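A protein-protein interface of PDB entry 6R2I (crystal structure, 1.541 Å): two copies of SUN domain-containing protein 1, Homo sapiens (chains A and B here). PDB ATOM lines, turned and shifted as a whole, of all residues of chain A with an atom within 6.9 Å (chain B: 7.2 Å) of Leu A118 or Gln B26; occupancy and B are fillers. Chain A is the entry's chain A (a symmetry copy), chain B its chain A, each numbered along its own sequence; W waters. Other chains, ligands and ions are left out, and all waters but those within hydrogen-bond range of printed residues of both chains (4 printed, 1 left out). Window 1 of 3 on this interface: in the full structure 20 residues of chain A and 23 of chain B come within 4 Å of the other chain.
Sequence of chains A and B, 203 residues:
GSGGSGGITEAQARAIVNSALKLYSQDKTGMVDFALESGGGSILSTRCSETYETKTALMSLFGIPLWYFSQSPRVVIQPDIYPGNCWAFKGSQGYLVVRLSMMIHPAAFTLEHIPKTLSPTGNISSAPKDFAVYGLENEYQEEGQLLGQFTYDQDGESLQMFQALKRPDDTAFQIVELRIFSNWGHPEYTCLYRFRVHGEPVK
OE1 of Glu A157 lies within salt-bridge range of NZ of Lys B22, 3.1 Å away. OE1 of Gln B26 sits at hydrogen-bond distance from OG1 of Thr A117 (3.0 Å). The side-chain carboxylate of Asp B27 lies within hydrogen-bond range of the side-chain hydroxyl of Tyr A82, at 3.3 Å. The backbone carbonyl oxygen (O) of Thr A117 sits close to the backbone NH (N) of Val B32 (3.4 Å).
O of Lys B22 sits at hydrogen-bond distance from OG of Ser B25 (2.7 Å). The side-chain carboxylate (OD1) of Asp B27 is in salt-bridge range of the guanidinium group (NH1) of Arg B196 (3.3 Å). The side-chain hydroxyl of Thr B29 sits at hydrogen-bond distance from the backbone NH of Met B31 (3.1 Å). The side-chain hydroxyl (OG1) of Thr A121 is in hydrogen-bond range of the side-chain hydroxyl (OG) of Ser A119 (3.0 Å).
Among the printed residues, pairs that only touch across the chains: Tyr A24 with Leu B21 (3.9 Å), Tyr A24 with Tyr B24 (3.7 Å), Tyr A24 with Ser B25 (3.2 Å), Tyr A82 with Leu B36 (3.98 Å), Pro A83 with Leu B36 (3.9 Å), Pro A115 with Gln B26 (3.8 Å), Thr A117 with Gly B30 (3.7 Å), Thr A117 with Met B31 (3.8 Å), Leu A118 with Gln B26 (3.8 Å), Leu A118 with Met B31 (3.5 Å), Leu A118 with Val B32 (3.6 Å), Ser A119 with Val B32 (3.4 Å) and Pro A120 with Val B32 (3.8 Å).
Of the printed residues of chain B, Leu A118 touches Gln B26, Met B31 and Val B32. Of chain A, only Pro A115, Thr A117 and Leu A118 come within 4 Å of Gln B26. Of the printed residues of chain B, Pro A120 touches Val B32 (3.8 Å). Of the printed residues of chain B, Pro A115 touches Gln B26. Printed residues of chain A within 4 Å of Met B31: Thr A117 (3.8 Å) and Leu A118 (3.5 Å). The nearest printed residue of chain B that does not touch Pro A83 is Asp B27 (6.3 Å).
Of the 16 printed residues of chain A, 9 touch a printed residue of chain B. Printed residues of chain A that touch a printed residue of chain B: Tyr A24, Tyr A82, Pro A83, Pro A115, Thr A117, Leu A118, Ser A119, Pro A120 and Glu A157. Hydrophobic or aromatic side chains of chain A that line the printed part of chain B: Tyr A24, Tyr A82, Pro A83, Pro A115 and Leu A118.
Tyr B24 touches its own counterpart, Tyr A24. 1 position is printed for both chains. Of the 17 pairs that touch across the chains among the printed residues, 1 has its exchanged pair printed and touching as well.
Water W1 lies within hydrogen-bond range of the side-chain carboxylate of Asp B27, the side-chain amino group of Lys B28, the guanidinium group of Arg B196 and the side-chain hydroxyl of Tyr A82. Water W2 lies within hydrogen-bond range of the side-chain hydroxyl of Tyr A82 (2.9 Å), the backbone NH of Asp B27 (3.2 Å) and the backbone carbonyl oxygen of Ser B25 (3.3 Å). Water W4 lies within hydrogen-bond range of the backbone carbonyl oxygen of Leu A118 and the backbone NH of Asp B33. Water W3 bridges OG of Ser B25 (3.3 Å) and OG of Ser A158 (3.5 Å).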
ATOM      1  N   TYR A  24      25.497  30.619   4.291  1.00  0.00           N
ATOM      2  CA  TYR A  24      24.051  30.693   4.087  1.00  0.00           C
ATOM      3  C   TYR A  24      23.715  31.262   2.708  1.00  0.00           C
ATOM      4  O   TYR A  24      22.819  30.743   2.004  1.00  0.00           O
ATOM      5  CB  TYR A  24      23.445  31.568   5.202  1.00  0.00           C
ATOM      6  CG  TYR A  24      21.925  31.624   5.251  1.00  0.00           C
ATOM      7  CD1 TYR A  24      21.209  32.650   4.628  1.00  0.00           C
ATOM      8  CD2 TYR A  24      21.211  30.672   5.952  1.00  0.00           C
ATOM      9  CE1 TYR A  24      19.829  32.705   4.707  1.00  0.00           C
ATOM     10  CE2 TYR A  24      19.826  30.718   6.020  1.00  0.00           C
ATOM     11  CZ  TYR A  24      19.140  31.723   5.382  1.00  0.00           C
ATOM     12  OH  TYR A  24      17.739  31.800   5.457  1.00  0.00           O
ATOM     13  N   ILE A  81      10.983  27.667  -1.401  1.00  0.00           N
ATOM     14  CA  ILE A  81      10.341  26.619  -0.616  1.00  0.00           C
ATOM     15  C   ILE A  81       9.345  27.195   0.395  1.00  0.00           C
ATOM     16  O   ILE A  81       9.156  26.617   1.467  1.00  0.00           O
ATOM     17  CB  ILE A  81      11.346  25.679   0.088  1.00  0.00           C
ATOM     18  CG1 ILE A  81      12.255  26.423   1.077  1.00  0.00           C
ATOM     19  CG2 ILE A  81      12.158  24.896  -0.977  1.00  0.00           C
ATOM     20  CD1 ILE A  81      12.821  25.505   2.156  1.00  0.00           C
ATOM     21  N   TYR A  82       8.674  28.306   0.060  1.00  0.00           N
ATOM     22  CA  TYR A  82       7.513  28.739   0.841  1.00  0.00           C
ATOM     23  C   TYR A  82       6.425  27.652   0.785  1.00  0.00           C
ATOM     24  O   TYR A  82       6.322  26.923  -0.213  1.00  0.00           O
ATOM     25  CB  TYR A  82       6.973  30.108   0.312  1.00  0.00           C
ATOM     26  CG  TYR A  82       7.742  31.267   0.937  1.00  0.00           C
ATOM     27  CD1 TYR A  82       9.004  31.614   0.491  1.00  0.00           C
ATOM     28  CD2 TYR A  82       7.222  31.982   2.017  1.00  0.00           C
ATOM     29  CE1 TYR A  82       9.741  32.631   1.103  1.00  0.00           C
ATOM     30  CE2 TYR A  82       7.967  32.998   2.652  1.00  0.00           C
ATOM     31  CZ  TYR A  82       9.228  33.308   2.186  1.00  0.00           C
ATOM     32  OH  TYR A  82       9.991  34.290   2.833  1.00  0.00           O
ATOM     33  N   PRO A  83       5.591  27.526   1.819  1.00  0.00           N
ATOM     34  CA  PRO A  83       4.501  26.529   1.782  1.00  0.00           C
ATOM     35  C   PRO A  83       3.689  26.569   0.494  1.00  0.00           C
ATOM     36  O   PRO A  83       3.257  27.638   0.040  1.00  0.00           O
ATOM     37  CB  PRO A  83       3.638  26.907   3.002  1.00  0.00           C
ATOM     38  CG  PRO A  83       4.662  27.475   3.991  1.00  0.00           C
ATOM     39  CD  PRO A  83       5.624  28.262   3.107  1.00  0.00           C
ATOM     40  N   ILE A 114       9.314  21.883   4.029  1.00  0.00           N
ATOM     41  CA  ILE A 114       9.042  22.917   5.033  1.00  0.00           C
ATOM     42  C   ILE A 114       9.101  22.365   6.458  1.00  0.00           C
ATOM     43  O   ILE A 114       8.834  21.178   6.695  1.00  0.00           O
ATOM     44  CB  ILE A 114       7.680  23.628   4.799  1.00  0.00           C
ATOM     45  CG1 ILE A 114       6.499  22.657   4.802  1.00  0.00           C
ATOM     46  CG2 ILE A 114       7.759  24.555   3.561  1.00  0.00           C
ATOM     47  CD1 ILE A 114       5.163  23.368   4.948  1.00  0.00           C
ATOM     48  N   PRO A 115       9.463  23.201   7.441  1.00  0.00           N
ATOM     49  CA  PRO A 115       9.332  22.781   8.849  1.00  0.00           C
ATOM     50  C   PRO A 115       7.876  22.805   9.316  1.00  0.00           C
ATOM     51  O   PRO A 115       7.055  23.573   8.795  1.00  0.00           O
ATOM     52  CB  PRO A 115      10.170  23.820   9.604  1.00  0.00           C
ATOM     53  CG  PRO A 115      10.047  25.075   8.751  1.00  0.00           C
ATOM     54  CD  PRO A 115       9.969  24.577   7.301  1.00  0.00           C
ATOM     55  N   LYS A 116       7.570  21.945  10.307  1.00  0.00           N
ATOM     56  CA  LYS A 116       6.225  21.853  10.883  1.00  0.00           C
ATOM     57  C   LYS A 116       5.737  23.197  11.416  1.00  0.00           C
ATOM     58  O   LYS A 116       4.541  23.502  11.330  1.00  0.00           O
ATOM     59  CB  LYS A 116       6.224  20.803  12.009  1.00  0.00           C
ATOM     60  CG  LYS A 116       4.909  20.453  12.623  1.00  0.00           C
ATOM     61  CD  LYS A 116       5.177  19.279  13.618  1.00  0.00           C
ATOM     62  CE  LYS A 116       3.972  18.800  14.411  1.00  0.00           C
ATOM     63  NZ  LYS A 116       4.296  17.821  15.490  1.00  0.00           N
ATOM     64  N   THR A 117       6.654  24.021  11.929  1.00  0.00           N
ATOM     65  CA  THR A 117       6.292  25.329  12.466  1.00  0.00           C
ATOM     66  C   THR A 117       5.705  26.272  11.424  1.00  0.00           C
ATOM     67  O   THR A 117       5.134  27.301  11.811  1.00  0.00           O
ATOM     68  CB  THR A 117       7.508  26.030  13.088  1.00  0.00           C
ATOM     69  OG1 THR A 117       8.574  26.051  12.126  1.00  0.00           O
ATOM     70  CG2 THR A 117       7.946  25.342  14.360  1.00  0.00           C
ATOM     71  N   LEU A 118       5.880  25.999  10.120  1.00  0.00           N
ATOM     72  CA  LEU A 118       5.311  26.854   9.069  1.00  0.00           C
ATOM     73  C   LEU A 118       4.155  26.206   8.312  1.00  0.00           C
ATOM     74  O   LEU A 118       3.570  26.856   7.426  1.00  0.00           O
ATOM     75  CB  LEU A 118       6.391  27.271   8.062  1.00  0.00           C
ATOM     76  CG  LEU A 118       7.556  28.126   8.597  1.00  0.00           C
ATOM     77  CD1 LEU A 118       8.530  28.458   7.462  1.00  0.00           C
ATOM     78  CD2 LEU A 118       7.004  29.381   9.282  1.00  0.00           C
ATOM     79  N   SER A 119       3.730  24.991   8.656  1.00  0.00           N
ATOM     80  CA  SER A 119       2.706  24.335   7.825  1.00  0.00           C
ATOM     81  C   SER A 119       1.292  24.835   8.144  1.00  0.00           C
ATOM     82  O   SER A 119       0.853  24.749   9.301  1.00  0.00           O
ATOM     83  CB  SER A 119       2.746  22.835   8.020  1.00  0.00           C
ATOM     84  OG  SER A 119       1.619  22.279   7.358  1.00  0.00           O
ATOM     85  N   PRO A 120       0.525  25.318   7.152  1.00  0.00           N
ATOM     86  CA  PRO A 120      -0.841  25.779   7.462  1.00  0.00           C
ATOM     87  C   PRO A 120      -1.835  24.652   7.741  1.00  0.00           C
ATOM     88  O   PRO A 120      -2.966  24.967   8.136  1.00  0.00           O
ATOM     89  CB  PRO A 120      -1.234  26.592   6.214  1.00  0.00           C
ATOM     90  CG  PRO A 120      -0.434  25.999   5.125  1.00  0.00           C
ATOM     91  CD  PRO A 120       0.896  25.634   5.761  1.00  0.00           C
ATOM     92  N   THR A 121      -1.468  23.374   7.566  1.00  0.00           N
ATOM     93  CA  THR A 121      -2.298  22.254   8.013  1.00  0.00           C
ATOM     94  C   THR A 121      -1.920  21.747   9.405  1.00  0.00           C
ATOM     95  O   THR A 121      -2.578  20.835   9.931  1.00  0.00           O
ATOM     96  CB  THR A 121      -2.206  21.069   7.035  1.00  0.00           C
ATOM     97  OG1 THR A 121      -0.847  20.635   6.938  1.00  0.00           O
ATOM     98  CG2 THR A 121      -2.673  21.456   5.632  1.00  0.00           C
ATOM     99  N   GLY A 122      -0.864  22.284  10.003  1.00  0.00           N
ATOM    100  CA  GLY A 122      -0.398  21.814  11.303  1.00  0.00           C
ATOM    101  C   GLY A 122       0.469  20.571  11.283  1.00  0.00           C
ATOM    102  O   GLY A 122       0.859  20.092  12.364  1.00  0.00           O
ATOM    103  N   ILE A 124       3.469  17.947   8.723  1.00  0.00           N
ATOM    104  CA  ILE A 124       4.219  17.661   7.498  1.00  0.00           C
ATOM    105  C   ILE A 124       4.053  16.174   7.151  1.00  0.00           C
ATOM    106  O   ILE A 124       4.989  15.504   6.691  1.00  0.00           O
ATOM    107  CB  ILE A 124       5.701  18.083   7.592  1.00  0.00           C
ATOM    108  CG1 ILE A 124       6.440  17.429   8.749  1.00  0.00           C
ATOM    109  CG2 ILE A 124       5.785  19.627   7.662  1.00  0.00           C
ATOM    110  CD1 ILE A 124       7.933  17.538   8.577  1.00  0.00           C
ATOM    111  N   GLU A 157      15.995  18.262  10.593  1.00  0.00           N
ATOM    112  CA  GLU A 157      16.014  19.622  10.062  1.00  0.00           C
ATOM    113  C   GLU A 157      15.333  19.706   8.680  1.00  0.00           C
ATOM    114  O   GLU A 157      15.149  18.710   7.974  1.00  0.00           O
ATOM    115  CB  GLU A 157      17.459  20.131   9.931  1.00  0.00           C
ATOM    116  CG  GLU A 157      18.282  20.121  11.241  1.00  0.00           C
ATOM    117  CD  GLU A 157      17.779  21.084  12.301  1.00  0.00           C
ATOM    118  OE1 GLU A 157      17.226  22.138  11.988  1.00  0.00           O
ATOM    119  OE2 GLU A 157      17.929  20.760  13.485  1.00  0.00           O
ATOM    120  N   SER A 158      14.982  20.938   8.287  1.00  0.00           N
ATOM    121  CA  SER A 158      14.326  21.164   6.995  1.00  0.00           C
ATOM    122  C   SER A 158      15.157  20.626   5.834  1.00  0.00           C
ATOM    123  O   SER A 158      14.630  19.912   4.947  1.00  0.00           O
ATOM    124  CB  SER A 158      14.057  22.679   6.830  1.00  0.00           C
ATOM    125  OG  SER A 158      13.582  23.034   5.519  1.00  0.00           O
ATOM    126  N   ALA B  20      19.988  31.693  15.296  1.00  0.00           N
ATOM    127  CA  ALA B  20      19.458  32.910  14.671  1.00  0.00           C
ATOM    128  C   ALA B  20      19.228  32.739  13.176  1.00  0.00           C
ATOM    129  O   ALA B  20      18.206  33.218  12.644  1.00  0.00           O
ATOM    130  CB  ALA B  20      20.406  34.082  14.922  1.00  0.00           C
ATOM    131  N   LEU B  21      20.155  32.062  12.470  1.00  0.00           N
ATOM    132  CA  LEU B  21      19.947  31.827  11.034  1.00  0.00           C
ATOM    133  C   LEU B  21      18.808  30.844  10.784  1.00  0.00           C
ATOM    134  O   LEU B  21      18.068  30.978   9.791  1.00  0.00           O
ATOM    135  CB  LEU B  21      21.245  31.316  10.385  1.00  0.00           C
ATOM    136  CG  LEU B  21      22.277  32.355  10.007  1.00  0.00           C
ATOM    137  CD1 LEU B  21      23.560  31.700   9.561  1.00  0.00           C
ATOM    138  CD2 LEU B  21      21.727  33.203   8.896  1.00  0.00           C
ATOM    139  N   LYS B  22      18.643  29.831  11.649  1.00  0.00           N
ATOM    140  CA  LYS B  22      17.491  28.936  11.496  1.00  0.00           C
ATOM    141  C   LYS B  22      16.176  29.701  11.598  1.00  0.00           C
ATOM    142  O   LYS B  22      15.266  29.515  10.760  1.00  0.00           O
ATOM    143  CB  LYS B  22      17.563  27.802  12.531  1.00  0.00           C
ATOM    144  CG  LYS B  22      16.384  26.819  12.496  1.00  0.00           C
ATOM    145  CD  LYS B  22      16.651  25.615  13.412  1.00  0.00           C
ATOM    146  CE  LYS B  22      15.439  24.689  13.520  1.00  0.00           C
ATOM    147  NZ  LYS B  22      15.705  23.481  14.362  1.00  0.00           N
ATOM    148  N   LEU B  23      16.045  30.561  12.626  1.00  0.00           N
ATOM    149  CA  LEU B  23      14.801  31.364  12.740  1.00  0.00           C
ATOM    150  C   LEU B  23      14.616  32.283  11.527  1.00  0.00           C
ATOM    151  O   LEU B  23      13.507  32.378  10.965  1.00  0.00           O
ATOM    152  CB  LEU B  23      14.810  32.173  14.038  1.00  0.00           C
ATOM    153  CG  LEU B  23      13.572  33.021  14.302  1.00  0.00           C
ATOM    154  CD1 LEU B  23      12.362  32.145  14.514  1.00  0.00           C
ATOM    155  CD2 LEU B  23      13.784  33.899  15.532  1.00  0.00           C
ATOM    156  N   TYR B  24      15.705  32.935  11.079  1.00  0.00           N
ATOM    157  CA  TYR B  24      15.632  33.806   9.907  1.00  0.00           C
ATOM    158  C   TYR B  24      15.089  33.054   8.691  1.00  0.00           C
ATOM    159  O   TYR B  24      14.237  33.581   7.942  1.00  0.00           O
ATOM    160  CB  TYR B  24      17.042  34.362   9.622  1.00  0.00           C
ATOM    161  CG  TYR B  24      17.130  35.423   8.535  1.00  0.00           C
ATOM    162  CD1 TYR B  24      17.445  35.094   7.214  1.00  0.00           C
ATOM    163  CD2 TYR B  24      16.936  36.756   8.839  1.00  0.00           C
ATOM    164  CE1 TYR B  24      17.553  36.072   6.243  1.00  0.00           C
ATOM    165  CE2 TYR B  24      17.030  37.737   7.863  1.00  0.00           C
ATOM    166  CZ  TYR B  24      17.320  37.389   6.566  1.00  0.00           C
ATOM    167  OH  TYR B  24      17.441  38.370   5.566  1.00  0.00           O
ATOM    168  N   SER B  25      15.567  31.818   8.490  1.00  0.00           N
ATOM    169  CA  SER B  25      15.177  30.990   7.332  1.00  0.00           C
ATOM    170  C   SER B  25      13.698  30.577   7.373  1.00  0.00           C
ATOM    171  O   SER B  25      13.138  30.225   6.323  1.00  0.00           O
ATOM    172  CB  SER B  25      16.069  29.738   7.257  1.00  0.00           C
ATOM    173  OG  SER B  25      15.643  28.714   8.163  1.00  0.00           O
ATOM    174  N   GLN B  26      13.073  30.600   8.540  1.00  0.00           N
ATOM    175  CA  GLN B  26      11.653  30.214   8.699  1.00  0.00           C
ATOM    176  C   GLN B  26      10.752  31.448   8.580  1.00  0.00           C
ATOM    177  O   GLN B  26      10.010  31.807   9.505  1.00  0.00           O
ATOM    178  CB  GLN B  26      11.450  29.510  10.044  1.00  0.00           C
ATOM    179  CG  GLN B  26      12.258  28.210  10.189  1.00  0.00           C
ATOM    180  CD  GLN B  26      11.833  27.372  11.401  1.00  0.00           C
ATOM    181  OE1 GLN B  26      11.016  27.810  12.207  1.00  0.00           O
ATOM    182  NE2 GLN B  26      12.406  26.179  11.547  1.00  0.00           N
ATOM    183  N   ASP B  27      10.826  32.120   7.423  1.00  0.00           N
ATOM    184  CA  ASP B  27      10.001  33.319   7.159  1.00  0.00           C
ATOM    185  C   ASP B  27      10.209  34.394   8.244  1.00  0.00           C
ATOM    186  O   ASP B  27       9.300  35.136   8.590  1.00  0.00           O
ATOM    187  CB  ASP B  27       8.520  32.910   7.041  1.00  0.00           C
ATOM    188  CG  ASP B  27       7.655  33.887   6.257  1.00  0.00           C
ATOM    189  OD1 ASP B  27       6.391  33.693   6.300  1.00  0.00           O
ATOM    190  OD2 ASP B  27       8.181  34.787   5.565  1.00  0.00           O
ATOM    191  N   LYS B  28      11.436  34.494   8.769  1.00  0.00           N
ATOM    192  CA  LYS B  28      11.888  35.447   9.790  1.00  0.00           C
ATOM    193  C   LYS B  28      11.272  35.254  11.184  1.00  0.00           C
ATOM    194  O   LYS B  28      11.964  35.525  12.185  1.00  0.00           O
ATOM    195  CB  LYS B  28      11.591  36.921   9.406  1.00  0.00           C
ATOM    196  CG  LYS B  28      11.934  37.391   7.992  1.00  0.00           C
ATOM    197  CD  LYS B  28      13.361  37.175   7.637  1.00  0.00           C
ATOM    198  CE  LYS B  28      13.663  37.721   6.204  1.00  0.00           C
ATOM    199  NZ  LYS B  28      13.008  36.918   5.079  1.00  0.00           N
ATOM    200  N   THR B  29      10.062  34.680  11.275  1.00  0.00           N
ATOM    201  CA  THR B  29       9.248  34.635  12.507  1.00  0.00           C
ATOM    202  C   THR B  29       9.116  33.249  13.128  1.00  0.00           C
ATOM    203  O   THR B  29       8.792  33.124  14.347  1.00  0.00           O
ATOM    204  CB  THR B  29       7.782  35.078  12.226  1.00  0.00           C
ATOM    205  OG1 THR B  29       7.178  34.138  11.328  1.00  0.00           O
ATOM    206  CG2 THR B  29       7.631  36.445  11.669  1.00  0.00           C
ATOM    207  N   GLY B  30       9.256  32.202  12.326  1.00  0.00           N
ATOM    208  CA  GLY B  30       8.958  30.863  12.802  1.00  0.00           C
ATOM    209  C   GLY B  30       7.498  30.559  13.073  1.00  0.00           C
ATOM    210  O   GLY B  30       7.223  29.600  13.808  1.00  0.00           O
ATOM    211  N   MET B  31       6.569  31.337  12.512  1.00  0.00           N
ATOM    212  CA  MET B  31       5.128  31.219  12.758  1.00  0.00           C
ATOM    213  C   MET B  31       4.361  31.035  11.448  1.00  0.00           C
ATOM    214  O   MET B  31       4.664  31.700  10.448  1.00  0.00           O
ATOM    215  CB  MET B  31       4.581  32.478  13.466  1.00  0.00           C
ATOM    216  CG  MET B  31       5.233  32.766  14.784  1.00  0.00           C
ATOM    217  SD  MET B  31       4.647  34.285  15.528  1.00  0.00           S
ATOM    218  CE  MET B  31       5.029  35.586  14.407  1.00  0.00           C
ATOM    219  N   VAL B  32       3.361  30.142  11.453  1.00  0.00           N
ATOM    220  CA  VAL B  32       2.500  29.983  10.275  1.00  0.00           C
ATOM    221  C   VAL B  32       1.864  31.329   9.913  1.00  0.00           C
ATOM    222  O   VAL B  32       1.318  32.027  10.785  1.00  0.00           O
ATOM    223  CB  VAL B  32       1.385  28.938  10.494  1.00  0.00           C
ATOM    224  CG1 VAL B  32       0.490  28.819   9.235  1.00  0.00           C
ATOM    225  CG2 VAL B  32       1.963  27.578  10.862  1.00  0.00           C
ATOM    226  N   ASP B  33       1.832  31.647   8.596  1.00  0.00           N
ATOM    227  CA  ASP B  33       1.082  32.783   8.035  1.00  0.00           C
ATOM    228  C   ASP B  33      -0.129  32.229   7.265  1.00  0.00           C
ATOM    229  O   ASP B  33       0.022  31.709   6.144  1.00  0.00           O
ATOM    230  CB  ASP B  33       1.944  33.626   7.108  1.00  0.00           C
ATOM    231  CG  ASP B  33       1.164  34.767   6.451  1.00  0.00           C
ATOM    232  OD1 ASP B  33      -0.004  35.009   6.832  1.00  0.00           O
ATOM    233  OD2 ASP B  33       1.745  35.387   5.524  1.00  0.00           O
ATOM    234  N   LEU B  36      -0.851  33.751   3.620  1.00  0.00           N
ATOM    235  CA  LEU B  36       0.098  33.587   2.513  1.00  0.00           C
ATOM    236  C   LEU B  36      -0.575  32.905   1.324  1.00  0.00           C
ATOM    237  O   LEU B  36      -1.143  31.826   1.454  1.00  0.00           O
ATOM    238  CB  LEU B  36       1.286  32.744   3.011  1.00  0.00           C
ATOM    239  CG  LEU B  36       2.433  32.482   2.029  1.00  0.00           C
ATOM    240  CD1 LEU B  36       3.242  33.753   1.827  1.00  0.00           C
ATOM    241  CD2 LEU B  36       3.324  31.312   2.494  1.00  0.00           C
ATOM    242  N   ARG B 196       0.495  39.638   7.274  1.00  0.00           N
ATOM    243  CA  ARG B 196       0.410  38.255   7.705  1.00  0.00           C
ATOM    244  C   ARG B 196      -0.604  38.109   8.834  1.00  0.00           C
ATOM    245  O   ARG B 196      -0.781  39.033   9.650  1.00  0.00           O
ATOM    246  CB  ARG B 196       1.783  37.715   8.232  1.00  0.00           C
ATOM    247  CG  ARG B 196       2.995  38.090   7.426  1.00  0.00           C
ATOM    248  CD  ARG B 196       4.234  37.390   7.977  1.00  0.00           C
ATOM    249  NE  ARG B 196       5.462  37.948   7.407  1.00  0.00           N
ATOM    250  CZ  ARG B 196       6.660  37.426   7.604  1.00  0.00           C
ATOM    251  NH1 ARG B 196       6.751  36.310   8.317  1.00  0.00           N
ATOM    252  NH2 ARG B 196       7.764  37.994   7.103  1.00  0.00           N
HETATM  253  O   HOH W   1      10.087  36.826   5.067  1.00  0.00           O
HETATM  254  O   HOH W   2      11.683  32.513   4.394  1.00  0.00           O
HETATM  255  O   HOH W   3      13.944  26.289   6.743  1.00  0.00           O
HETATM  256  O   HOH W   4       3.290  29.703   6.742  1.00  0.00           O
